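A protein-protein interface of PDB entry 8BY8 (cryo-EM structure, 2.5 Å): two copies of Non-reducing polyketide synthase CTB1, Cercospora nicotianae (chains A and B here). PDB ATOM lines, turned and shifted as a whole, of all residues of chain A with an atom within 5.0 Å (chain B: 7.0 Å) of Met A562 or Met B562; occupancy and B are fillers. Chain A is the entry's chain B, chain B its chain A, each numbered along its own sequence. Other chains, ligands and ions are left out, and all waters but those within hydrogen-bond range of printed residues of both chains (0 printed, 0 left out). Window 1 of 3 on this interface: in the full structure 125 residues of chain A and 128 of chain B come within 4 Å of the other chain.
The side-chain hydroxyl (OH) of Tyr B547 lies within hydrogen-bond range of a ring nitrogen (ND1) of His A561 (3.2 Å). A ring nitrogen (ND1) of His B561 is in hydrogen-bond range of the side-chain hydroxyl (OH) of Tyr A547 (3.4 Å). OE2 of Glu B571 lies within hydrogen-bond range of NE2 of His A561 (3.4 Å). The side-chain amide nitrogen (ND2) of Asn A565 sits at hydrogen-bond distance from the side-chain carboxylate (OE2) of Glu B571 (2.8 Å).
N of Tyr B503 sits at hydrogen-bond distance from O of Tyr B547, 3.2 Å away. The backbone carbonyl oxygen of Tyr B503 sits at hydrogen-bond distance from the backbone NH of Ile B549 (3.0 Å). The backbone NH (N) of Thr B551 is in hydrogen-bond range of the side-chain hydroxyl (OG) of Ser B555 (3.2 Å). The backbone carbonyl oxygen (O) of His B561 sits at hydrogen-bond distance from the side-chain amide nitrogen (ND2) of Asn B565 (3.4 Å). O of Ala B566 is in hydrogen-bond range of N of Glu B571 (3.3 Å). O of His A561 sits close to ND2 of Asn A565 (3.4 Å).
Among the printed residues, merely in contact across the chains: Tyr A547 with Thr B551 (3.9 Å), Tyr A547 with Ala B558 (3.7 Å), Tyr A547 with Met B562 (3.4 Å), Ile A549 with Thr B548 (3.7 Å), Ile A549 with Ile B549 (3.6 Å), Ile A549 with Met B562 (3.9 Å), Ala A558 with Tyr B547 (3.5 Å), Met A562 with Tyr B547 (3.4 Å), Met A562 with Ile B549 (3.5 Å) and Met A562 with Met B562 (3.8 Å).
Met B562 touches three residues of chain A. Printed residues of chain B within 4 Å of Asn A565: Glu B571 (2.8 Å). Of the printed residues of chain A, Thr B548 touches Ile A549 (3.7 Å). Of the printed residues of chain A, Thr B551 touches Tyr A547 (3.9 Å). Of the printed residues of chain A, Ile B549 touches Ile A549 and Met A562. Leu B560 touches none of the printed residues of chain A. The nearest residue of chain B that does not touch Met A562 is Trp B502 (4.7 Å). The nearest residue of chain A that does not touch Met B562 is Trp A502 (4.6 Å). The nearest printed residue of chain A that does not touch Thr B548 is Met A562 (5.5 Å).
Hydrophobic or aromatic side chains of chain B that line the printed part of chain A: Tyr B547, Ile B549, Ala B558, His B561 and Met B562. Along chain B the printed residues that touch a printed residue of chain A span positions 547 to 571. Hydrophobic or aromatic side chains of chain A within 4 Å of the printed part of chain B: Tyr A547, Ile A549, Ala A558, His A561 and Met A562. Among the printed residues, no Asp or Glu carboxylate lies within 4 Å of a Lys or Arg side-chain nitrogen of the other chain.
Tyr A547 touches Ala B558, and with the chains exchanged Ala A558 touches Tyr B547. Tyr A547 touches Met B562, and with the chains exchanged Met A562 touches Tyr B547. Ile A549 touches Met B562, and with the chains exchanged Met A562 touches Ile B549. Met B562 touches its own counterpart, Met A562.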
ATOM      1  N   TRP A 502      24.907 -11.565  -0.594  1.00  0.00           N
ATOM      2  CA  TRP A 502      26.193 -11.503  -1.271  1.00  0.00           C
ATOM      3  C   TRP A 502      27.296 -11.368  -0.233  1.00  0.00           C
ATOM      4  O   TRP A 502      27.181 -10.566   0.698  1.00  0.00           O
ATOM      5  CB  TRP A 502      26.244 -10.321  -2.238  1.00  0.00           C
ATOM      6  CG  TRP A 502      25.335 -10.445  -3.411  1.00  0.00           C
ATOM      7  CD1 TRP A 502      25.679 -10.839  -4.666  1.00  0.00           C
ATOM      8  CD2 TRP A 502      23.931 -10.161  -3.450  1.00  0.00           C
ATOM      9  NE1 TRP A 502      24.581 -10.819  -5.488  1.00  0.00           N
ATOM     10  CE2 TRP A 502      23.493 -10.408  -4.765  1.00  0.00           C
ATOM     11  CE3 TRP A 502      23.001  -9.724  -2.502  1.00  0.00           C
ATOM     12  CZ2 TRP A 502      22.171 -10.233  -5.157  1.00  0.00           C
ATOM     13  CZ3 TRP A 502      21.687  -9.550  -2.894  1.00  0.00           C
ATOM     14  CH2 TRP A 502      21.285  -9.805  -4.209  1.00  0.00           C
ATOM     15  N   TYR A 547      25.450 -15.592  -3.042  1.00  0.00           N
ATOM     16  CA  TYR A 547      26.685 -15.564  -3.814  1.00  0.00           C
ATOM     17  C   TYR A 547      27.895 -15.292  -2.932  1.00  0.00           C
ATOM     18  O   TYR A 547      27.813 -14.568  -1.934  1.00  0.00           O
ATOM     19  CB  TYR A 547      26.629 -14.494  -4.903  1.00  0.00           C
ATOM     20  CG  TYR A 547      25.519 -14.672  -5.909  1.00  0.00           C
ATOM     21  CD1 TYR A 547      25.613 -15.620  -6.916  1.00  0.00           C
ATOM     22  CD2 TYR A 547      24.387 -13.875  -5.866  1.00  0.00           C
ATOM     23  CE1 TYR A 547      24.604 -15.775  -7.844  1.00  0.00           C
ATOM     24  CE2 TYR A 547      23.377 -14.023  -6.790  1.00  0.00           C
ATOM     25  CZ  TYR A 547      23.490 -14.974  -7.775  1.00  0.00           C
ATOM     26  OH  TYR A 547      22.481 -15.123  -8.696  1.00  0.00           O
ATOM     27  N   ILE A 549      31.955 -13.974  -3.641  1.00  0.00           N
ATOM     28  CA  ILE A 549      32.738 -13.295  -4.661  1.00  0.00           C
ATOM     29  C   ILE A 549      34.208 -13.350  -4.272  1.00  0.00           C
ATOM     30  O   ILE A 549      34.564 -13.373  -3.092  1.00  0.00           O
ATOM     31  CB  ILE A 549      32.281 -11.836  -4.852  1.00  0.00           C
ATOM     32  CG1 ILE A 549      30.757 -11.765  -4.981  1.00  0.00           C
ATOM     33  CG2 ILE A 549      32.951 -11.222  -6.064  1.00  0.00           C
ATOM     34  CD1 ILE A 549      30.186 -12.637  -6.061  1.00  0.00           C
ATOM     35  N   ALA A 558      33.159  -5.428  -4.751  1.00  0.00           N
ATOM     36  CA  ALA A 558      32.573  -6.122  -5.894  1.00  0.00           C
ATOM     37  C   ALA A 558      31.253  -6.785  -5.515  1.00  0.00           C
ATOM     38  O   ALA A 558      30.275  -6.728  -6.273  1.00  0.00           O
ATOM     39  CB  ALA A 558      33.557  -7.158  -6.434  1.00  0.00           C
ATOM     40  N   ALA A 559      31.209  -7.424  -4.343  1.00  0.00           N
ATOM     41  CA  ALA A 559      29.965  -8.017  -3.864  1.00  0.00           C
ATOM     42  C   ALA A 559      28.907  -6.949  -3.627  1.00  0.00           C
ATOM     43  O   ALA A 559      27.724  -7.163  -3.910  1.00  0.00           O
ATOM     44  CB  ALA A 559      30.224  -8.808  -2.583  1.00  0.00           C
ATOM     45  N   LEU A 560      29.311  -5.796  -3.092  1.00  0.00           N
ATOM     46  CA  LEU A 560      28.369  -4.693  -2.928  1.00  0.00           C
ATOM     47  C   LEU A 560      27.846  -4.216  -4.275  1.00  0.00           C
ATOM     48  O   LEU A 560      26.663  -3.889  -4.410  1.00  0.00           O
ATOM     49  CB  LEU A 560      29.035  -3.542  -2.173  1.00  0.00           C
ATOM     50  CG  LEU A 560      28.206  -2.265  -2.011  1.00  0.00           C
ATOM     51  CD1 LEU A 560      26.925  -2.530  -1.235  1.00  0.00           C
ATOM     52  CD2 LEU A 560      29.030  -1.193  -1.328  1.00  0.00           C
ATOM     53  N   HIS A 561      28.715  -4.167  -5.285  1.00  0.00           N
ATOM     54  CA  HIS A 561      28.281  -3.773  -6.622  1.00  0.00           C
ATOM     55  C   HIS A 561      27.260  -4.758  -7.174  1.00  0.00           C
ATOM     56  O   HIS A 561      26.251  -4.359  -7.763  1.00  0.00           O
ATOM     57  CB  HIS A 561      29.493  -3.677  -7.547  1.00  0.00           C
ATOM     58  CG  HIS A 561      29.192  -3.081  -8.886  1.00  0.00           C
ATOM     59  ND1 HIS A 561      30.089  -3.108  -9.931  1.00  0.00           N
ATOM     60  CD2 HIS A 561      28.095  -2.437  -9.349  1.00  0.00           C
ATOM     61  CE1 HIS A 561      29.557  -2.511 -10.981  1.00  0.00           C
ATOM     62  NE2 HIS A 561      28.348  -2.094 -10.655  1.00  0.00           N
ATOM     63  N   MET A 562      27.507  -6.055  -6.986  1.00  0.00           N
ATOM     64  CA  MET A 562      26.560  -7.065  -7.449  1.00  0.00           C
ATOM     65  C   MET A 562      25.230  -6.963  -6.711  1.00  0.00           C
ATOM     66  O   MET A 562      24.159  -7.073  -7.321  1.00  0.00           O
ATOM     67  CB  MET A 562      27.167  -8.454  -7.275  1.00  0.00           C
ATOM     68  CG  MET A 562      28.264  -8.759  -8.274  1.00  0.00           C
ATOM     69  SD  MET A 562      29.323 -10.109  -7.746  1.00  0.00           S
ATOM     70  CE  MET A 562      30.379 -10.291  -9.177  1.00  0.00           C
ATOM     71  N   ALA A 563      25.277  -6.758  -5.392  1.00  0.00           N
ATOM     72  CA  ALA A 563      24.049  -6.608  -4.620  1.00  0.00           C
ATOM     73  C   ALA A 563      23.269  -5.378  -5.063  1.00  0.00           C
ATOM     74  O   ALA A 563      22.037  -5.414  -5.158  1.00  0.00           O
ATOM     75  CB  ALA A 563      24.377  -6.523  -3.131  1.00  0.00           C
ATOM     76  N   CYS A 564      23.969  -4.276  -5.332  1.00  0.00           N
ATOM     77  CA  CYS A 564      23.299  -3.071  -5.803  1.00  0.00           C
ATOM     78  C   CYS A 564      22.721  -3.265  -7.197  1.00  0.00           C
ATOM     79  O   CYS A 564      21.657  -2.721  -7.501  1.00  0.00           O
ATOM     80  CB  CYS A 564      24.267  -1.888  -5.784  1.00  0.00           C
ATOM     81  SG  CYS A 564      24.747  -1.344  -4.130  1.00  0.00           S
ATOM     82  N   ASN A 565      23.399  -4.030  -8.056  1.00  0.00           N
ATOM     83  CA  ASN A 565      22.824  -4.359  -9.356  1.00  0.00           C
ATOM     84  C   ASN A 565      21.547  -5.171  -9.196  1.00  0.00           C
ATOM     85  O   ASN A 565      20.552  -4.923  -9.887  1.00  0.00           O
ATOM     86  CB  ASN A 565      23.837  -5.130 -10.205  1.00  0.00           C
ATOM     87  CG  ASN A 565      24.844  -4.224 -10.880  1.00  0.00           C
ATOM     88  OD1 ASN A 565      24.568  -3.054 -11.143  1.00  0.00           O
ATOM     89  ND2 ASN A 565      26.020  -4.763 -11.175  1.00  0.00           N
ATOM     90  N   ALA A 566      21.559  -6.148  -8.288  1.00  0.00           N
ATOM     91  CA  ALA A 566      20.356  -6.934  -8.033  1.00  0.00           C
ATOM     92  C   ALA A 566      19.223  -6.054  -7.523  1.00  0.00           C
ATOM     93  O   ALA A 566      18.072  -6.202  -7.947  1.00  0.00           O
ATOM     94  CB  ALA A 566      20.661  -8.049  -7.036  1.00  0.00           C
ATOM     95  N   TRP B 502      33.608 -12.540 -16.587  1.00  0.00           N
ATOM     96  CA  TRP B 502      33.106 -13.297 -15.450  1.00  0.00           C
ATOM     97  C   TRP B 502      33.541 -14.752 -15.555  1.00  0.00           C
ATOM     98  O   TRP B 502      33.706 -15.293 -16.651  1.00  0.00           O
ATOM     99  CB  TRP B 502      31.584 -13.221 -15.380  1.00  0.00           C
ATOM    100  CG  TRP B 502      31.057 -11.868 -15.051  1.00  0.00           C
ATOM    101  CD1 TRP B 502      30.646 -11.429 -13.831  1.00  0.00           C
ATOM    102  CD2 TRP B 502      30.872 -10.773 -15.956  1.00  0.00           C
ATOM    103  NE1 TRP B 502      30.213 -10.129 -13.916  1.00  0.00           N
ATOM    104  CE2 TRP B 502      30.344  -9.702 -15.211  1.00  0.00           C
ATOM    105  CE3 TRP B 502      31.103 -10.593 -17.323  1.00  0.00           C
ATOM    106  CZ2 TRP B 502      30.042  -8.471 -15.783  1.00  0.00           C
ATOM    107  CZ3 TRP B 502      30.801  -9.369 -17.890  1.00  0.00           C
ATOM    108  CH2 TRP B 502      30.278  -8.325 -17.121  1.00  0.00           C
ATOM    109  N   TYR B 503      33.727 -15.383 -14.400  1.00  0.00           N
ATOM    110  CA  TYR B 503      34.163 -16.768 -14.342  1.00  0.00           C
ATOM    111  C   TYR B 503      33.557 -17.432 -13.115  1.00  0.00           C
ATOM    112  O   TYR B 503      33.046 -16.769 -12.210  1.00  0.00           O
ATOM    113  CB  TYR B 503      35.691 -16.868 -14.305  1.00  0.00           C
ATOM    114  CG  TYR B 503      36.310 -17.367 -15.590  1.00  0.00           C
ATOM    115  CD1 TYR B 503      36.448 -16.529 -16.689  1.00  0.00           C
ATOM    116  CD2 TYR B 503      36.768 -18.672 -15.701  1.00  0.00           C
ATOM    117  CE1 TYR B 503      37.017 -16.979 -17.863  1.00  0.00           C
ATOM    118  CE2 TYR B 503      37.337 -19.131 -16.871  1.00  0.00           C
ATOM    119  CZ  TYR B 503      37.460 -18.281 -17.948  1.00  0.00           C
ATOM    120  OH  TYR B 503      38.027 -18.735 -19.115  1.00  0.00           O
ATOM    121  N   SER B 546      36.062  -7.733 -13.831  1.00  0.00           N
ATOM    122  CA  SER B 546      36.746  -9.025 -13.821  1.00  0.00           C
ATOM    123  C   SER B 546      36.425  -9.703 -12.489  1.00  0.00           C
ATOM    124  O   SER B 546      37.039  -9.385 -11.467  1.00  0.00           O
ATOM    125  CB  SER B 546      38.245  -8.847 -14.013  1.00  0.00           C
ATOM    126  OG  SER B 546      38.931 -10.075 -13.874  1.00  0.00           O
ATOM    127  N   TYR B 547      35.480 -10.639 -12.516  1.00  0.00           N
ATOM    128  CA  TYR B 547      34.938 -11.250 -11.311  1.00  0.00           C
ATOM    129  C   TYR B 547      35.146 -12.757 -11.326  1.00  0.00           C
ATOM    130  O   TYR B 547      35.254 -13.378 -12.387  1.00  0.00           O
ATOM    131  CB  TYR B 547      33.442 -10.964 -11.170  1.00  0.00           C
ATOM    132  CG  TYR B 547      33.069  -9.504 -11.107  1.00  0.00           C
ATOM    133  CD1 TYR B 547      33.292  -8.758  -9.959  1.00  0.00           C
ATOM    134  CD2 TYR B 547      32.466  -8.878 -12.185  1.00  0.00           C
ATOM    135  CE1 TYR B 547      32.937  -7.427  -9.895  1.00  0.00           C
ATOM    136  CE2 TYR B 547      32.108  -7.549 -12.128  1.00  0.00           C
ATOM    137  CZ  TYR B 547      32.346  -6.829 -10.982  1.00  0.00           C
ATOM    138  OH  TYR B 547      31.991  -5.504 -10.922  1.00  0.00           O
ATOM    139  N   THR B 548      35.205 -13.335 -10.130  1.00  0.00           N
ATOM    140  CA  THR B 548      35.149 -14.775  -9.933  1.00  0.00           C
ATOM    141  C   THR B 548      33.998 -15.083  -8.986  1.00  0.00           C
ATOM    142  O   THR B 548      33.833 -14.416  -7.961  1.00  0.00           O
ATOM    143  CB  THR B 548      36.459 -15.317  -9.358  1.00  0.00           C
ATOM    144  OG1 THR B 548      37.552 -14.915 -10.190  1.00  0.00           O
ATOM    145  CG2 THR B 548      36.422 -16.830  -9.287  1.00  0.00           C
ATOM    146  N   ILE B 549      33.202 -16.091  -9.331  1.00  0.00           N
ATOM    147  CA  ILE B 549      31.988 -16.420  -8.595  1.00  0.00           C
ATOM    148  C   ILE B 549      32.121 -17.820  -8.019  1.00  0.00           C
ATOM    149  O   ILE B 549      32.577 -18.743  -8.703  1.00  0.00           O
ATOM    150  CB  ILE B 549      30.740 -16.316  -9.492  1.00  0.00           C
ATOM    151  CG1 ILE B 549      30.746 -14.991 -10.259  1.00  0.00           C
ATOM    152  CG2 ILE B 549      29.481 -16.447  -8.659  1.00  0.00           C
ATOM    153  CD1 ILE B 549      30.924 -13.780  -9.397  1.00  0.00           C
ATOM    154  N   ASP B 550      31.726 -17.972  -6.751  1.00  0.00           N
ATOM    155  CA  ASP B 550      31.833 -19.239  -6.022  1.00  0.00           C
ATOM    156  C   ASP B 550      30.478 -19.562  -5.394  1.00  0.00           C
ATOM    157  O   ASP B 550      30.210 -19.189  -4.250  1.00  0.00           O
ATOM    158  CB  ASP B 550      32.933 -19.164  -4.970  1.00  0.00           C
ATOM    159  CG  ASP B 550      33.206 -20.500  -4.322  1.00  0.00           C
ATOM    160  OD1 ASP B 550      32.324 -21.379  -4.369  1.00  0.00           O
ATOM    161  OD2 ASP B 550      34.306 -20.675  -3.761  1.00  0.00           O
ATOM    162  N   THR B 551      29.627 -20.261  -6.143  1.00  0.00           N
ATOM    163  CA  THR B 551      28.397 -20.851  -5.612  1.00  0.00           C
ATOM    164  C   THR B 551      28.459 -22.374  -5.633  1.00  0.00           C
ATOM    165  O   THR B 551      27.471 -23.046  -5.933  1.00  0.00           O
ATOM    166  CB  THR B 551      27.182 -20.349  -6.387  1.00  0.00           C
ATOM    167  OG1 THR B 551      27.586 -19.910  -7.686  1.00  0.00           O
ATOM    168  CG2 THR B 551      26.510 -19.201  -5.654  1.00  0.00           C
ATOM    169  N   SER B 555      28.450 -22.440  -9.826  1.00  0.00           N
ATOM    170  CA  SER B 555      29.211 -21.214 -10.053  1.00  0.00           C
ATOM    171  C   SER B 555      29.120 -20.754 -11.501  1.00  0.00           C
ATOM    172  O   SER B 555      28.747 -19.607 -11.781  1.00  0.00           O
ATOM    173  CB  SER B 555      30.673 -21.443  -9.673  1.00  0.00           C
ATOM    174  OG  SER B 555      30.774 -22.131  -8.441  1.00  0.00           O
ATOM    175  N   LEU B 557      27.001 -21.261 -13.816  1.00  0.00           N
ATOM    176  CA  LEU B 557      25.710 -20.686 -14.166  1.00  0.00           C
ATOM    177  C   LEU B 557      25.469 -19.399 -13.391  1.00  0.00           C
ATOM    178  O   LEU B 557      25.025 -18.397 -13.962  1.00  0.00           O
ATOM    179  CB  LEU B 557      24.586 -21.697 -13.916  1.00  0.00           C
ATOM    180  CG  LEU B 557      23.551 -21.783 -15.044  1.00  0.00           C
ATOM    181  CD1 LEU B 557      24.230 -22.103 -16.369  1.00  0.00           C
ATOM    182  CD2 LEU B 557      22.496 -22.823 -14.732  1.00  0.00           C
ATOM    183  N   ALA B 558      25.801 -19.394 -12.096  1.00  0.00           N
ATOM    184  CA  ALA B 558      25.680 -18.171 -11.311  1.00  0.00           C
ATOM    185  C   ALA B 558      26.484 -17.047 -11.949  1.00  0.00           C
ATOM    186  O   ALA B 558      25.957 -15.959 -12.211  1.00  0.00           O
ATOM    187  CB  ALA B 558      26.141 -18.421  -9.874  1.00  0.00           C
ATOM    188  N   ALA B 559      27.761 -17.310 -12.239  1.00  0.00           N
ATOM    189  CA  ALA B 559      28.578 -16.339 -12.954  1.00  0.00           C
ATOM    190  C   ALA B 559      27.886 -15.898 -14.233  1.00  0.00           C
ATOM    191  O   ALA B 559      27.814 -14.702 -14.538  1.00  0.00           O
ATOM    192  CB  ALA B 559      29.950 -16.938 -13.263  1.00  0.00           C
ATOM    193  N   LEU B 560      27.342 -16.858 -14.983  1.00  0.00           N
ATOM    194  CA  LEU B 560      26.615 -16.515 -16.198  1.00  0.00           C
ATOM    195  C   LEU B 560      25.557 -15.465 -15.895  1.00  0.00           C
ATOM    196  O   LEU B 560      25.503 -14.411 -16.540  1.00  0.00           O
ATOM    197  CB  LEU B 560      25.984 -17.774 -16.794  1.00  0.00           C
ATOM    198  CG  LEU B 560      25.866 -17.852 -18.316  1.00  0.00           C
ATOM    199  CD1 LEU B 560      25.233 -19.170 -18.722  1.00  0.00           C
ATOM    200  CD2 LEU B 560      25.065 -16.687 -18.861  1.00  0.00           C
ATOM    201  N   HIS B 561      24.746 -15.714 -14.865  1.00  0.00           N
ATOM    202  CA  HIS B 561      23.722 -14.751 -14.476  1.00  0.00           C
ATOM    203  C   HIS B 561      24.334 -13.368 -14.300  1.00  0.00           C
ATOM    204  O   HIS B 561      23.864 -12.385 -14.890  1.00  0.00           O
ATOM    205  CB  HIS B 561      23.042 -15.215 -13.185  1.00  0.00           C
ATOM    206  CG  HIS B 561      21.772 -14.488 -12.868  1.00  0.00           C
ATOM    207  ND1 HIS B 561      21.063 -14.710 -11.708  1.00  0.00           N
ATOM    208  CD2 HIS B 561      21.077 -13.552 -13.558  1.00  0.00           C
ATOM    209  CE1 HIS B 561      19.990 -13.940 -11.694  1.00  0.00           C
ATOM    210  NE2 HIS B 561      19.976 -13.227 -12.805  1.00  0.00           N
ATOM    211  N   MET B 562      25.431 -13.287 -13.539  1.00  0.00           N
ATOM    212  CA  MET B 562      26.090 -12.003 -13.326  1.00  0.00           C
ATOM    213  C   MET B 562      26.339 -11.313 -14.657  1.00  0.00           C
ATOM    214  O   MET B 562      25.905 -10.175 -14.875  1.00  0.00           O
ATOM    215  CB  MET B 562      27.417 -12.204 -12.591  1.00  0.00           C
ATOM    216  CG  MET B 562      27.347 -12.999 -11.297  1.00  0.00           C
ATOM    217  SD  MET B 562      26.580 -12.109  -9.934  1.00  0.00           S
ATOM    218  CE  MET B 562      27.165 -13.086  -8.553  1.00  0.00           C
ATOM    219  N   ALA B 563      26.989 -12.021 -15.583  1.00  0.00           N
ATOM    220  CA  ALA B 563      27.325 -11.420 -16.866  1.00  0.00           C
ATOM    221  C   ALA B 563      26.080 -10.860 -17.529  1.00  0.00           C
ATOM    222  O   ALA B 563      26.060  -9.706 -17.973  1.00  0.00           O
ATOM    223  CB  ALA B 563      28.004 -12.453 -17.763  1.00  0.00           C
ATOM    224  N   CYS B 564      25.003 -11.648 -17.547  1.00  0.00           N
ATOM    225  CA  CYS B 564      23.795 -11.193 -18.223  1.00  0.00           C
ATOM    226  C   CYS B 564      23.280  -9.915 -17.586  1.00  0.00           C
ATOM    227  O   CYS B 564      22.900  -8.971 -18.290  1.00  0.00           O
ATOM    228  CB  CYS B 564      22.730 -12.287 -18.190  1.00  0.00           C
ATOM    229  SG  CYS B 564      23.215 -13.803 -19.036  1.00  0.00           S
ATOM    230  N   ASN B 565      23.301  -9.846 -16.253  1.00  0.00           N
ATOM    231  CA  ASN B 565      22.881  -8.623 -15.580  1.00  0.00           C
ATOM    232  C   ASN B 565      23.670  -7.436 -16.108  1.00  0.00           C
ATOM    233  O   ASN B 565      23.095  -6.405 -16.475  1.00  0.00           O
ATOM    234  CB  ASN B 565      23.056  -8.768 -14.068  1.00  0.00           C
ATOM    235  CG  ASN B 565      21.982  -9.629 -13.437  1.00  0.00           C
ATOM    236  OD1 ASN B 565      20.811  -9.549 -13.806  1.00  0.00           O
ATOM    237  ND2 ASN B 565      22.374 -10.460 -12.479  1.00  0.00           N
ATOM    238  N   ALA B 566      24.993  -7.585 -16.198  1.00  0.00           N
ATOM    239  CA  ALA B 566      25.806  -6.523 -16.772  1.00  0.00           C
ATOM    240  C   ALA B 566      25.335  -6.199 -18.181  1.00  0.00           C
ATOM    241  O   ALA B 566      25.072  -5.036 -18.510  1.00  0.00           O
ATOM    242  CB  ALA B 566      27.279  -6.927 -16.770  1.00  0.00           C
ATOM    243  N   LEU B 567      25.176  -7.229 -19.018  1.00  0.00           N
ATOM    244  CA  LEU B 567      24.683  -7.002 -20.370  1.00  0.00           C
ATOM    245  C   LEU B 567      23.336  -6.298 -20.341  1.00  0.00           C
ATOM    246  O   LEU B 567      23.047  -5.460 -21.203  1.00  0.00           O
ATOM    247  CB  LEU B 567      24.579  -8.328 -21.124  1.00  0.00           C
ATOM    248  CG  LEU B 567      25.821  -8.825 -21.877  1.00  0.00           C
ATOM    249  CD1 LEU B 567      26.278  -7.814 -22.917  1.00  0.00           C
ATOM    250  CD2 LEU B 567      26.954  -9.150 -20.925  1.00  0.00           C
ATOM    251  N   TRP B 568      22.499  -6.620 -19.354  1.00  0.00           N
ATOM    252  CA  TRP B 568      21.192  -5.985 -19.275  1.00  0.00           C
ATOM    253  C   TRP B 568      21.279  -4.567 -18.729  1.00  0.00           C
ATOM    254  O   TRP B 568      20.426  -3.732 -19.053  1.00  0.00           O
ATOM    255  CB  TRP B 568      20.244  -6.830 -18.418  1.00  0.00           C
ATOM    256  CG  TRP B 568      19.633  -7.990 -19.158  1.00  0.00           C
ATOM    257  CD1 TRP B 568      19.052  -7.959 -20.393  1.00  0.00           C
ATOM    258  CD2 TRP B 568      19.525  -9.345 -18.702  1.00  0.00           C
ATOM    259  NE1 TRP B 568      18.598  -9.208 -20.737  1.00  0.00           N
ATOM    260  CE2 TRP B 568      18.876 -10.077 -19.715  1.00  0.00           C
ATOM    261  CE3 TRP B 568      19.918 -10.011 -17.536  1.00  0.00           C
ATOM    262  CZ2 TRP B 568      18.611 -11.439 -19.598  1.00  0.00           C
ATOM    263  CZ3 TRP B 568      19.652 -11.362 -17.423  1.00  0.00           C
ATOM    264  CH2 TRP B 568      19.007 -12.062 -18.448  1.00  0.00           C
ATOM    265  N   GLU B 571      26.779  -2.179 -18.386  1.00  0.00           N
ATOM    266  CA  GLU B 571      28.154  -2.033 -17.921  1.00  0.00           C
ATOM    267  C   GLU B 571      29.141  -2.462 -18.995  1.00  0.00           C
ATOM    268  O   GLU B 571      30.189  -1.830 -19.175  1.00  0.00           O
ATOM    269  CB  GLU B 571      28.362  -2.849 -16.646  1.00  0.00           C
ATOM    270  CG  GLU B 571      27.490  -2.414 -15.486  1.00  0.00           C
ATOM    271  CD  GLU B 571      27.589  -3.353 -14.304  1.00  0.00           C
ATOM    272  OE1 GLU B 571      28.520  -4.184 -14.277  1.00  0.00           O
ATOM    273  OE2 GLU B 571      26.730  -3.263 -13.403  1.00  0.00           O
ATOM    274  N   VAL B 577      32.346 -15.379 -20.463  1.00  0.00           N
ATOM    275  CA  VAL B 577      31.865 -16.124 -19.304  1.00  0.00           C
ATOM    276  C   VAL B 577      32.470 -17.519 -19.341  1.00  0.00           C
ATOM    277  O   VAL B 577      32.308 -18.248 -20.324  1.00  0.00           O
ATOM    278  CB  VAL B 577      30.331 -16.186 -19.279  1.00  0.00           C
ATOM    279  CG1 VAL B 577      29.853 -17.166 -18.229  1.00  0.00           C
ATOM    280  CG2 VAL B 577      29.755 -14.811 -19.011  1.00  0.00           C
ATOM    281  N   ILE B 645      17.053 -15.899 -17.086  1.00  0.00           N
ATOM    282  CA  ILE B 645      17.774 -16.657 -16.072  1.00  0.00           C
ATOM    283  C   ILE B 645      17.400 -16.080 -14.716  1.00  0.00           C
ATOM    284  O   ILE B 645      17.104 -14.889 -14.595  1.00  0.00           O
ATOM    285  CB  ILE B 645      19.304 -16.626 -16.325  1.00  0.00           C
ATOM    286  CG1 ILE B 645      20.045 -17.372 -15.216  1.00  0.00           C
ATOM    287  CG2 ILE B 645      19.802 -15.192 -16.445  1.00  0.00           C
ATOM    288  CD1 ILE B 645      21.466 -17.732 -15.567  1.00  0.00           C
